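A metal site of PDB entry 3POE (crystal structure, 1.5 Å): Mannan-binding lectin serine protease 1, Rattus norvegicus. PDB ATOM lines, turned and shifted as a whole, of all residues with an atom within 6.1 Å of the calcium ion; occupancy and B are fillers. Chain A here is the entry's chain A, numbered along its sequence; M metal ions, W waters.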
ATOM      1  N   TYR A  25      22.108  -9.146  -9.083  1.00  0.00           N
ATOM      2  CA  TYR A  25      21.619  -7.955  -8.415  1.00  0.00           C
ATOM      3  C   TYR A  25      20.207  -7.652  -8.933  1.00  0.00           C
ATOM      4  O   TYR A  25      19.851  -7.990 -10.064  1.00  0.00           O
ATOM      5  CB  TYR A  25      22.580  -6.765  -8.592  1.00  0.00           C
ATOM      6  CG  TYR A  25      23.110  -6.444  -9.969  1.00  0.00           C
ATOM      7  CD1 TYR A  25      22.334  -5.828 -10.933  1.00  0.00           C
ATOM      8  CD2 TYR A  25      24.425  -6.649 -10.284  1.00  0.00           C
ATOM      9  CE1 TYR A  25      22.837  -5.510 -12.142  1.00  0.00           C
ATOM     10  CE2 TYR A  25      24.961  -6.341 -11.487  1.00  0.00           C
ATOM     11  CZ  TYR A  25      24.188  -5.746 -12.439  1.00  0.00           C
ATOM     12  OH  TYR A  25      24.707  -5.337 -13.651  1.00  0.00           O
ATOM     13  N   GLU A  54      26.844  -5.357 -15.927  1.00  0.00           N
ATOM     14  CA  GLU A  54      26.542  -5.252 -17.352  1.00  0.00           C
ATOM     15  C   GLU A  54      27.204  -4.040 -17.974  1.00  0.00           C
ATOM     16  O   GLU A  54      27.217  -2.953 -17.392  1.00  0.00           O
ATOM     17  CB  GLU A  54      25.026  -5.130 -17.560  1.00  0.00           C
ATOM     18  CG  GLU A  54      24.567  -5.421 -18.954  1.00  0.00           C
ATOM     19  CD  GLU A  54      23.080  -5.391 -19.081  1.00  0.00           C
ATOM     20  OE1 GLU A  54      22.408  -4.647 -18.343  1.00  0.00           O
ATOM     21  OE2 GLU A  54      22.569  -6.107 -19.969  1.00  0.00           O
ATOM     22  N   TYR A  63      24.300   2.476 -17.757  1.00  0.00           N
ATOM     23  CA  TYR A  63      23.059   2.166 -17.042  1.00  0.00           C
ATOM     24  C   TYR A  63      23.234   1.253 -15.830  1.00  0.00           C
ATOM     25  O   TYR A  63      22.458   1.312 -14.892  1.00  0.00           O
ATOM     26  CB  TYR A  63      22.065   1.610 -17.966  1.00  0.00           C
ATOM     27  CG  TYR A  63      21.745   2.490 -19.149  1.00  0.00           C
ATOM     28  CD1 TYR A  63      21.340   3.819 -18.994  1.00  0.00           C
ATOM     29  CD2 TYR A  63      21.920   2.019 -20.430  1.00  0.00           C
ATOM     30  CE1 TYR A  63      21.131   4.648 -20.095  1.00  0.00           C
ATOM     31  CE2 TYR A  63      21.613   2.843 -21.547  1.00  0.00           C
ATOM     32  CZ  TYR A  63      21.240   4.178 -21.367  1.00  0.00           C
ATOM     33  OH  TYR A  63      20.996   4.974 -22.492  1.00  0.00           O
ATOM     34  N   ASP A  64      24.254   0.370 -15.925  1.00  0.00           N
ATOM     35  CA  ASP A  64      24.665  -0.471 -14.791  1.00  0.00           C
ATOM     36  C   ASP A  64      26.102  -0.055 -14.498  1.00  0.00           C
ATOM     37  O   ASP A  64      26.963  -0.177 -15.378  1.00  0.00           O
ATOM     38  CB  ASP A  64      24.645  -1.963 -15.074  1.00  0.00           C
ATOM     39  CG  ASP A  64      23.279  -2.583 -15.303  1.00  0.00           C
ATOM     40  OD1 ASP A  64      22.336  -1.940 -15.768  1.00  0.00           O
ATOM     41  OD2 ASP A  64      23.147  -3.827 -15.122  1.00  0.00           O
ATOM     42  N   SER A 100      21.518   0.069 -11.644  1.00  0.00           N
ATOM     43  CA  SER A 100      21.258  -0.969 -12.613  1.00  0.00           C
ATOM     44  C   SER A 100      19.903  -0.685 -13.273  1.00  0.00           C
ATOM     45  O   SER A 100      18.988  -0.136 -12.652  1.00  0.00           O
ATOM     46  CB  SER A 100      21.255  -2.415 -12.064  1.00  0.00           C
ATOM     47  OG  SER A 100      20.139  -2.546 -11.219  1.00  0.00           O
ATOM     48  N   ASP A 101      19.742  -1.183 -14.494  1.00  0.00           N
ATOM     49  CA  ASP A 101      18.549  -0.985 -15.265  1.00  0.00           C
ATOM     50  C   ASP A 101      17.631  -2.212 -15.191  1.00  0.00           C
ATOM     51  O   ASP A 101      17.704  -3.000 -14.246  1.00  0.00           O
ATOM     52  CB  ASP A 101      18.851  -0.557 -16.675  1.00  0.00           C
ATOM     53  CG  ASP A 101      19.565  -1.637 -17.517  1.00  0.00           C
ATOM     54  OD1 ASP A 101      19.686  -2.829 -17.046  1.00  0.00           O
ATOM     55  OD2 ASP A 101      19.929  -1.317 -18.667  1.00  0.00           O
ATOM     56  N   ASN A 102      16.731  -2.340 -16.178  1.00  0.00           N
ATOM     57  CA  ASN A 102      15.744  -3.398 -16.156  1.00  0.00           C
ATOM     58  C   ASN A 102      16.038  -4.581 -17.038  1.00  0.00           C
ATOM     59  O   ASN A 102      15.106  -5.452 -17.292  1.00  0.00           O
ATOM     60  CB  ASN A 102      14.361  -2.806 -16.515  1.00  0.00           C
ATOM     61  CG  ASN A 102      13.819  -1.897 -15.463  1.00  0.00           C
ATOM     62  OD1 ASN A 102      13.189  -0.808 -15.744  1.00  0.00           O
ATOM     63  ND2 ASN A 102      13.998  -2.284 -14.242  1.00  0.00           N
ATOM     64  N   SER A 103      17.241  -4.691 -17.539  1.00  0.00           N
ATOM     65  CA  SER A 103      17.555  -5.882 -18.285  1.00  0.00           C
ATOM     66  C   SER A 103      18.839  -6.534 -17.887  1.00  0.00           C
ATOM     67  O   SER A 103      19.671  -5.934 -17.266  1.00  0.00           O
ATOM     68  CB  SER A 103      17.483  -5.625 -19.754  1.00  0.00           C
ATOM     69  OG  SER A 103      18.427  -4.730 -20.169  1.00  0.00           O
ATOM     70  N   GLY A 104      18.953  -7.815 -18.254  1.00  0.00           N
ATOM     71  CA  GLY A 104      20.164  -8.585 -17.961  1.00  0.00           C
ATOM     72  C   GLY A 104      20.104  -9.277 -16.637  1.00  0.00           C
ATOM     73  O   GLY A 104      19.146  -9.057 -15.850  1.00  0.00           O
ATOM     74  N   GLU A 105      21.137 -10.100 -16.339  1.00  0.00           N
ATOM     75  CA  GLU A 105      21.237 -10.897 -15.085  1.00  0.00           C
ATOM     76  C   GLU A 105      22.612 -11.067 -14.399  1.00  0.00           C
ATOM     77  O   GLU A 105      23.006 -12.112 -13.843  1.00  0.00           O
ATOM     78  CB  GLU A 105      20.691 -12.288 -15.266  1.00  0.00           C
ATOM     79  CG  GLU A 105      19.174 -12.406 -15.297  1.00  0.00           C
ATOM     80  CD  GLU A 105      18.365 -11.530 -14.305  1.00  0.00           C
ATOM     81  OE1 GLU A 105      17.187 -11.263 -14.651  1.00  0.00           O
ATOM     82  OE2 GLU A 105      18.830 -11.112 -13.222  1.00  0.00           O
ATOM     83  N   ASN A 106      23.278  -9.994 -14.209  1.00  0.00           N
ATOM     84  CA  ASN A 106      24.667  -9.949 -13.748  1.00  0.00           C
ATOM     85  C   ASN A 106      24.745  -9.983 -12.231  1.00  0.00           C
ATOM     86  O   ASN A 106      23.809  -9.577 -11.524  1.00  0.00           O
ATOM     87  CB  ASN A 106      25.348  -8.628 -14.292  1.00  0.00           C
ATOM     88  CG  ASN A 106      25.342  -8.600 -15.807  1.00  0.00           C
ATOM     89  OD1 ASN A 106      26.331  -9.031 -16.464  1.00  0.00           O
ATOM     90  ND2 ASN A 106      24.221  -8.201 -16.376  1.00  0.00           N
HETATM   91 CA    CA M   1      21.260  -4.424 -16.409  1.00  0.00          CA
HETATM   92  O   HOH W   1      22.145  -6.599 -15.541  1.00  0.00           O
HETATM   93  O   HOH W   2      19.998  -4.582 -14.348  1.00  0.00           O
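Within 4 Å of the calcium ion: Glu 54, Asp 64, Asp 101 and Ser 103.
The calcium ion is bound by the side-chain carboxylate (OE1) of Glu 54, the side-chain carboxylate (OD1) of Asp 101, the backbone carbonyl oxygen (O) of Ser 103, the side-chain carboxylate (OD2) of Asp 64, water W2, water W1 and the side-chain carboxylate (OD1) of Asp 64.
The calcium ion has seven donor atoms within binding distance.
Water W1 bridges ND2 of Asn 106 (2.8 Å) and OH of Tyr 25 (3.4 Å).
The backbone NH (N) of Glu 54 is in hydrogen-bond range of the side-chain hydroxyl (OH) of Tyr 25, at 3.1 Å.
The side-chain carboxylate of Asp 64 sits close to the side-chain hydroxyl of Tyr 25 (2.6 Å).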
